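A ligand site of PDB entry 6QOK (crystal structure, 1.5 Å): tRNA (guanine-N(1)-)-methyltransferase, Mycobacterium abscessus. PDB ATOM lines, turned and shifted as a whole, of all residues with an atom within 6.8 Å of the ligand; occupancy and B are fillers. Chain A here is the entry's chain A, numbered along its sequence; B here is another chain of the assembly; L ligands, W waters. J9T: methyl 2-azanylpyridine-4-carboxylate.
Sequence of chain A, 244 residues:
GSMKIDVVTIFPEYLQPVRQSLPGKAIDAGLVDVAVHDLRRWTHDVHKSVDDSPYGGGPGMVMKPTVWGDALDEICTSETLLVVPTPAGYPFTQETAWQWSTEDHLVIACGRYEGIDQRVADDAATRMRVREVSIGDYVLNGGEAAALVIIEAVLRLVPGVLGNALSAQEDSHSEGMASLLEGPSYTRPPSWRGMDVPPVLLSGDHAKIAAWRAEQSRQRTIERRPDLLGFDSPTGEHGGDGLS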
ATOM      1  N   VAL A  84       6.393  12.641  24.994  1.00  0.00           N
ATOM      2  CA  VAL A  84       6.066  11.925  26.219  1.00  0.00           C
ATOM      3  C   VAL A  84       4.566  11.946  26.446  1.00  0.00           C
ATOM      4  O   VAL A  84       4.021  12.943  26.937  1.00  0.00           O
ATOM      5  CB  VAL A  84       6.775  12.538  27.449  1.00  0.00           C
ATOM      6  CG1 VAL A  84       6.561  11.652  28.661  1.00  0.00           C
ATOM      7  CG2 VAL A  84       8.273  12.699  27.171  1.00  0.00           C
ATOM      8  N   PRO A  85       3.852  10.855  26.093  1.00  0.00           N
ATOM      9  CA  PRO A  85       2.411  10.831  26.367  1.00  0.00           C
ATOM     10  C   PRO A  85       2.118  10.785  27.867  1.00  0.00           C
ATOM     11  O   PRO A  85       2.668   9.964  28.602  1.00  0.00           O
ATOM     12  CB  PRO A  85       1.923   9.542  25.682  1.00  0.00           C
ATOM     13  CG  PRO A  85       2.977   9.255  24.635  1.00  0.00           C
ATOM     14  CD  PRO A  85       4.277   9.718  25.256  1.00  0.00           C
ATOM     15  N   THR A  86       1.259  11.685  28.308  1.00  0.00           N
ATOM     16  CA  THR A  86       0.865  11.719  29.711  1.00  0.00           C
ATOM     17  C   THR A  86      -0.478  12.411  29.842  1.00  0.00           C
ATOM     18  O   THR A  86      -0.738  13.350  29.115  1.00  0.00           O
ATOM     19  CB  THR A  86       1.918  12.444  30.592  1.00  0.00           C
ATOM     20  OG1 THR A  86       1.348  12.770  31.865  1.00  0.00           O
ATOM     21  CG2 THR A  86       2.449  13.711  29.912  1.00  0.00           C
ATOM     22  N   PRO A  87      -1.334  11.944  30.758  1.00  0.00           N
ATOM     23  CA  PRO A  87      -2.615  12.626  30.899  1.00  0.00           C
ATOM     24  C   PRO A  87      -2.438  14.047  31.415  1.00  0.00           C
ATOM     25  O   PRO A  87      -3.379  14.844  31.313  1.00  0.00           O
ATOM     26  CB  PRO A  87      -3.390  11.749  31.902  1.00  0.00           C
ATOM     27  CG  PRO A  87      -2.369  10.992  32.628  1.00  0.00           C
ATOM     28  CD  PRO A  87      -1.139  10.869  31.752  1.00  0.00           C
ATOM     29  N   ALA A  88      -1.249  14.362  31.924  1.00  0.00           N
ATOM     30  CA  ALA A  88      -0.984  15.713  32.409  1.00  0.00           C
ATOM     31  C   ALA A  88      -0.337  16.601  31.351  1.00  0.00           C
ATOM     32  O   ALA A  88       0.186  17.654  31.670  1.00  0.00           O
ATOM     33  CB  ALA A  88      -0.090  15.651  33.662  1.00  0.00           C
ATOM     34  N   GLY A  89      -0.345  16.162  30.082  1.00  0.00           N
ATOM     35  CA  GLY A  89       0.329  16.909  29.037  1.00  0.00           C
ATOM     36  C   GLY A  89      -0.467  18.058  28.430  1.00  0.00           C
ATOM     37  O   GLY A  89      -1.643  18.273  28.737  1.00  0.00           O
ATOM     38  N   GLY A 111       5.419   5.705  29.304  1.00  0.00           N
ATOM     39  CA  GLY A 111       5.492   5.424  30.733  1.00  0.00           C
ATOM     40  C   GLY A 111       4.160   5.077  31.358  1.00  0.00           C
ATOM     41  O   GLY A 111       3.094   5.319  30.782  1.00  0.00           O
ATOM     42  N   ARG A 112       4.219   4.530  32.568  1.00  0.00           N
ATOM     43  CA  ARG A 112       3.017   4.313  33.375  1.00  0.00           C
ATOM     44  C   ARG A 112       2.382   5.648  33.797  1.00  0.00           C
ATOM     45  O   ARG A 112       3.061   6.662  33.866  1.00  0.00           O
ATOM     46  CB  ARG A 112       3.373   3.490  34.607  1.00  0.00           C
ATOM     47  CG  ARG A 112       4.342   4.215  35.529  1.00  0.00           C
ATOM     48  N   TYR A 113       1.080   5.639  34.111  1.00  0.00           N
ATOM     49  CA  TYR A 113       0.385   6.906  34.328  1.00  0.00           C
ATOM     50  C   TYR A 113       0.879   7.678  35.559  1.00  0.00           C
ATOM     51  O   TYR A 113       0.733   8.902  35.611  1.00  0.00           O
ATOM     52  CB  TYR A 113      -1.133   6.692  34.413  1.00  0.00           C
ATOM     53  CG  TYR A 113      -1.640   6.135  35.713  1.00  0.00           C
ATOM     54  CD1 TYR A 113      -1.646   4.774  35.956  1.00  0.00           C
ATOM     55  CD2 TYR A 113      -2.136   6.983  36.705  1.00  0.00           C
ATOM     56  CE1 TYR A 113      -2.110   4.252  37.152  1.00  0.00           C
ATOM     57  CE2 TYR A 113      -2.604   6.477  37.901  1.00  0.00           C
ATOM     58  CZ  TYR A 113      -2.590   5.115  38.121  1.00  0.00           C
ATOM     59  OH  TYR A 113      -3.058   4.609  39.317  1.00  0.00           O
ATOM     60  N   GLU A 114       1.485   6.991  36.524  1.00  0.00           N
ATOM     61  CA  GLU A 114       2.017   7.680  37.699  1.00  0.00           C
ATOM     62  C   GLU A 114       3.205   8.537  37.314  1.00  0.00           C
ATOM     63  O   GLU A 114       3.595   9.457  38.054  1.00  0.00           O
ATOM     64  CB  GLU A 114       2.413   6.708  38.808  1.00  0.00           C
ATOM     65  CG  GLU A 114       1.280   5.839  39.318  1.00  0.00           C
ATOM     66  CD  GLU A 114       1.153   4.539  38.558  1.00  0.00           C
ATOM     67  OE1 GLU A 114       0.610   3.567  39.130  1.00  0.00           O
ATOM     68  OE2 GLU A 114       1.602   4.479  37.386  1.00  0.00           O
ATOM     69  N   VAL A 133       2.485  15.380  26.116  1.00  0.00           N
ATOM     70  CA  VAL A 133       1.167  15.596  25.525  1.00  0.00           C
ATOM     71  C   VAL A 133       0.127  14.591  25.978  1.00  0.00           C
ATOM     72  O   VAL A 133       0.444  13.428  26.237  1.00  0.00           O
ATOM     73  CB  VAL A 133       1.206  15.560  23.976  1.00  0.00           C
ATOM     74  CG1 VAL A 133       2.049  16.700  23.430  1.00  0.00           C
ATOM     75  CG2 VAL A 133       1.723  14.212  23.471  1.00  0.00           C
ATOM     76  N   SER A 134      -1.115  15.061  26.064  1.00  0.00           N
ATOM     77  CA  SER A 134      -2.269  14.219  26.340  1.00  0.00           C
ATOM     78  C   SER A 134      -3.096  14.053  25.080  1.00  0.00           C
ATOM     79  O   SER A 134      -3.295  15.011  24.334  1.00  0.00           O
ATOM     80  CB  SER A 134      -3.124  14.820  27.448  1.00  0.00           C
ATOM     81  OG  SER A 134      -4.367  14.152  27.522  1.00  0.00           O
ATOM     82  N   ILE A 135      -3.611  12.852  24.868  1.00  0.00           N
ATOM     83  CA  ILE A 135      -4.476  12.638  23.691  1.00  0.00           C
ATOM     84  C   ILE A 135      -5.968  12.771  24.011  1.00  0.00           C
ATOM     85  O   ILE A 135      -6.811  12.573  23.130  1.00  0.00           O
ATOM     86  CB  ILE A 135      -4.222  11.250  23.036  1.00  0.00           C
ATOM     87  CG1 ILE A 135      -4.542  10.094  23.986  1.00  0.00           C
ATOM     88  CG2 ILE A 135      -2.780  11.153  22.519  1.00  0.00           C
ATOM     89  CD1 ILE A 135      -4.808   8.775  23.222  1.00  0.00           C
ATOM     90  N   GLY A 136      -6.315  13.116  25.246  1.00  0.00           N
ATOM     91  CA  GLY A 136      -7.720  13.299  25.592  1.00  0.00           C
ATOM     92  C   GLY A 136      -7.890  13.363  27.099  1.00  0.00           C
ATOM     93  O   GLY A 136      -6.927  13.239  27.846  1.00  0.00           O
ATOM     94  N   ASP A 137      -9.133  13.556  27.540  1.00  0.00           N
ATOM     95  CA  ASP A 137      -9.398  13.767  28.953  1.00  0.00           C
ATOM     96  C   ASP A 137      -9.767  12.472  29.644  1.00  0.00           C
ATOM     97  O   ASP A 137     -10.907  12.290  30.075  1.00  0.00           O
ATOM     98  CB  ASP A 137     -10.534  14.791  29.122  1.00  0.00           C
ATOM     99  CG  ASP A 137     -10.118  16.190  28.728  1.00  0.00           C
ATOM    100  OD1 ASP A 137      -8.913  16.493  28.782  1.00  0.00           O
ATOM    101  OD2 ASP A 137     -11.006  16.990  28.352  1.00  0.00           O
ATOM    102  N   TYR A 138      -8.809  11.564  29.715  1.00  0.00           N
ATOM    103  CA  TYR A 138      -8.970  10.274  30.391  1.00  0.00           C
ATOM    104  C   TYR A 138      -7.586   9.751  30.752  1.00  0.00           C
ATOM    105  O   TYR A 138      -6.550  10.189  30.208  1.00  0.00           O
ATOM    106  CB  TYR A 138      -9.709   9.264  29.503  1.00  0.00           C
ATOM    107  CG  TYR A 138      -9.294   9.364  28.055  1.00  0.00           C
ATOM    108  CD1 TYR A 138      -8.110   8.796  27.610  1.00  0.00           C
ATOM    109  CD2 TYR A 138     -10.072  10.074  27.151  1.00  0.00           C
ATOM    110  CE1 TYR A 138      -7.705   8.934  26.296  1.00  0.00           C
ATOM    111  CE2 TYR A 138      -9.682  10.202  25.824  1.00  0.00           C
ATOM    112  CZ  TYR A 138      -8.498   9.630  25.415  1.00  0.00           C
ATOM    113  OH  TYR A 138      -8.079   9.748  24.115  1.00  0.00           O
ATOM    114  N   VAL A 139      -7.572   8.799  31.674  1.00  0.00           N
ATOM    115  CA  VAL A 139      -6.337   8.193  32.136  1.00  0.00           C
ATOM    116  C   VAL A 139      -6.247   6.762  31.623  1.00  0.00           C
ATOM    117  O   VAL A 139      -7.246   6.040  31.619  1.00  0.00           O
ATOM    118  CB  VAL A 139      -6.273   8.217  33.678  1.00  0.00           C
ATOM    119  CG1 VAL A 139      -5.047   7.457  34.184  1.00  0.00           C
ATOM    120  CG2 VAL A 139      -6.217   9.662  34.166  1.00  0.00           C
ATOM    121  N   LEU A 140      -5.066   6.371  31.161  1.00  0.00           N
ATOM    122  CA  LEU A 140      -4.772   4.996  30.780  1.00  0.00           C
ATOM    123  C   LEU A 140      -3.788   4.455  31.788  1.00  0.00           C
ATOM    124  O   LEU A 140      -3.214   5.215  32.545  1.00  0.00           O
ATOM    125  CB  LEU A 140      -4.169   4.944  29.369  1.00  0.00           C
ATOM    126  CG  LEU A 140      -4.955   5.754  28.332  1.00  0.00           C
ATOM    127  CD1 LEU A 140      -4.202   5.792  26.998  1.00  0.00           C
ATOM    128  CD2 LEU A 140      -6.331   5.136  28.144  1.00  0.00           C
ATOM    129  N   ASN A 141      -3.565   3.149  31.798  1.00  0.00           N
ATOM    130  CA  ASN A 141      -2.510   2.637  32.680  1.00  0.00           C
ATOM    131  C   ASN A 141      -1.106   2.935  32.195  1.00  0.00           C
ATOM    132  O   ASN A 141      -0.191   3.105  33.008  1.00  0.00           O
ATOM    133  CB  ASN A 141      -2.676   1.132  32.877  1.00  0.00           C
ATOM    134  CG  ASN A 141      -3.981   0.792  33.528  1.00  0.00           C
ATOM    135  OD1 ASN A 141      -4.287   1.278  34.624  1.00  0.00           O
ATOM    136  ND2 ASN A 141      -4.802   0.002  32.847  1.00  0.00           N
ATOM    137  N   GLY A 142      -0.930   2.992  30.880  1.00  0.00           N
ATOM    138  CA  GLY A 142       0.365   3.249  30.291  1.00  0.00           C
ATOM    139  C   GLY A 142       0.222   4.065  29.023  1.00  0.00           C
ATOM    140  O   GLY A 142      -0.881   4.242  28.489  1.00  0.00           O
ATOM    141  N   GLY A 143       1.347   4.578  28.540  1.00  0.00           N
ATOM    142  CA  GLY A 143       1.303   5.462  27.382  1.00  0.00           C
ATOM    143  C   GLY A 143       1.227   4.768  26.032  1.00  0.00           C
ATOM    144  O   GLY A 143       1.105   5.450  25.019  1.00  0.00           O
ATOM    145  N   GLU A 144       1.273   3.433  26.007  1.00  0.00           N
ATOM    146  CA  GLU A 144       1.379   2.695  24.753  1.00  0.00           C
ATOM    147  C   GLU A 144       0.206   2.935  23.802  1.00  0.00           C
ATOM    148  O   GLU A 144       0.423   3.178  22.624  1.00  0.00           O
ATOM    149  CB  GLU A 144       1.522   1.192  25.042  1.00  0.00           C
ATOM    150  CG  GLU A 144       2.932   0.797  25.501  1.00  0.00           C
ATOM    151  CD  GLU A 144       3.208   1.102  26.964  1.00  0.00           C
ATOM    152  OE1 GLU A 144       2.257   1.384  27.734  1.00  0.00           O
ATOM    153  OE2 GLU A 144       4.393   1.086  27.348  1.00  0.00           O
ATOM    154  N   ALA A 146      -1.718   5.501  23.699  1.00  0.00           N
ATOM    155  CA  ALA A 146      -1.585   6.882  23.233  1.00  0.00           C
ATOM    156  C   ALA A 146      -0.497   7.011  22.176  1.00  0.00           C
ATOM    157  O   ALA A 146      -0.660   7.769  21.225  1.00  0.00           O
ATOM    158  CB  ALA A 146      -1.289   7.809  24.413  1.00  0.00           C
ATOM    159  N   ALA A 147       0.608   6.288  22.334  1.00  0.00           N
ATOM    160  CA  ALA A 147       1.645   6.241  21.318  1.00  0.00           C
ATOM    161  C   ALA A 147       1.093   5.755  19.985  1.00  0.00           C
ATOM    162  O   ALA A 147       1.420   6.323  18.930  1.00  0.00           O
ATOM    163  CB  ALA A 147       2.796   5.361  21.758  1.00  0.00           C
ATOM    164  N   ILE A 150      -0.956   8.607  18.441  1.00  0.00           N
ATOM    165  CA  ILE A 150      -0.067   9.647  17.932  1.00  0.00           C
ATOM    166  C   ILE A 150       0.643   9.215  16.640  1.00  0.00           C
ATOM    167  O   ILE A 150       0.687   9.976  15.660  1.00  0.00           O
ATOM    168  CB  ILE A 150       0.967  10.043  19.002  1.00  0.00           C
ATOM    169  CG1 ILE A 150       0.260  10.813  20.119  1.00  0.00           C
ATOM    170  CG2 ILE A 150       2.071  10.908  18.387  1.00  0.00           C
ATOM    171  CD1 ILE A 150       1.111  10.932  21.387  1.00  0.00           C
ATOM    172  N   GLU B 152      -8.697   0.288  27.183  1.00  0.00           N
ATOM    173  CA  GLU B 152      -7.787   0.486  28.307  1.00  0.00           C
ATOM    174  C   GLU B 152      -8.377   1.440  29.357  1.00  0.00           C
ATOM    175  O   GLU B 152      -8.243   1.206  30.552  1.00  0.00           O
ATOM    176  CB  GLU B 152      -6.432   1.004  27.828  1.00  0.00           C
ATOM    177  CG  GLU B 152      -5.453   1.183  28.970  1.00  0.00           C
ATOM    178  CD  GLU B 152      -4.030   0.843  28.581  1.00  0.00           C
ATOM    179  OE1 GLU B 152      -3.843   0.335  27.458  1.00  0.00           O
ATOM    180  OE2 GLU B 152      -3.112   1.073  29.390  1.00  0.00           O
HETATM  181  C01 J9T L   1      -0.175   6.759  30.827  1.00  0.00           C
HETATM  182  O02 J9T L   1      -0.524   7.559  29.724  1.00  0.00           O
HETATM  183  C03 J9T L   1      -1.808   8.060  29.796  1.00  0.00           C
HETATM  184  O04 J9T L   1      -2.554   7.729  30.683  1.00  0.00           O
HETATM  185  C05 J9T L   1      -2.212   9.057  28.758  1.00  0.00           C
HETATM  186  C06 J9T L   1      -1.303   9.474  27.776  1.00  0.00           C
HETATM  187  C07 J9T L   1      -1.687  10.425  26.852  1.00  0.00           C
HETATM  188  N08 J9T L   1      -2.933  10.917  26.901  1.00  0.00           N
HETATM  189  C09 J9T L   1      -3.798  10.507  27.822  1.00  0.00           C
HETATM  190  N10 J9T L   1      -5.086  11.059  27.829  1.00  0.00           N
HETATM  191  C11 J9T L   1      -3.481   9.572  28.793  1.00  0.00           C
HETATM  192  O   HOH W   1       2.551   8.665  31.554  1.00  0.00           O
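O of Gly 136 sits at hydrogen-bond distance from OG of Ser 134 (2.7 Å).
O of Ile 135 is in hydrogen-bond range of OH of Tyr 138 (3.2 Å).
The backbone NH (N) of Gly 142 is in hydrogen-bond range of the side-chain carboxylate (OE2) of Glu 152 of chain B (3.3 Å).
The backbone NH (N) of Thr 86 is in hydrogen-bond range of the backbone carbonyl oxygen (O) of Val 133, at 2.8 Å.
OG1 of Thr 86 sits close to N of Ala 88.
The backbone carbonyl oxygen (O) of Gly 111 is in hydrogen-bond range of the backbone NH (N) of Gly 143, at 2.9 Å.
The backbone NH (N) of Tyr 113 is in hydrogen-bond range of the backbone carbonyl oxygen (O) of Asn 141, 3.0 Å away.
N of Val 133 sits at hydrogen-bond distance from O of Val 84 (3.0 Å).
Pro 85 touches the ligand.
N of Thr 86 touches C06 of the ligand, at 3.4 Å.
Pro 87 touches the ligand (CD to C03, 3.5 Å).
Gly 111 touches the ligand (O to C01, 3.6 Å).
Tyr 113 touches the ligand (CA to C01, 3.5 Å).
O of Val 133 touches C07 of the ligand, at 3.7 Å.
Val 139 touches the ligand.
Gly 142 touches the ligand.
Gly 143 touches the ligand (N to C01, 3.5 Å).
Ala 146 touches the ligand.
15 residues have an atom within 4 Å of the ligand: Pro 85, Thr 86, Pro 87, Gly 111, Tyr 113, Val 133, Ser 134, Ile 135, Gly 136, Tyr 138, Val 139, Leu 140, Gly 142, Gly 143 and Ala 146.
O of Gly 136 sits at hydrogen-bond distance from N10 of the ligand.
The backbone NH (N) of Ile 135 is in hydrogen-bond range of a nitrogen (N08) of the ligand, 2.9 Å away.
The backbone NH of Leu 140 sits at hydrogen-bond distance from an oxygen (O04) of the ligand, 2.9 Å away.
The backbone carbonyl oxygen (O) of Tyr 138 is in hydrogen-bond range of a nitrogen (N10) of the ligand, at 2.9 Å.
N10 of the ligand lies within hydrogen-bond range of OG of Ser 134 (3.2 Å).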
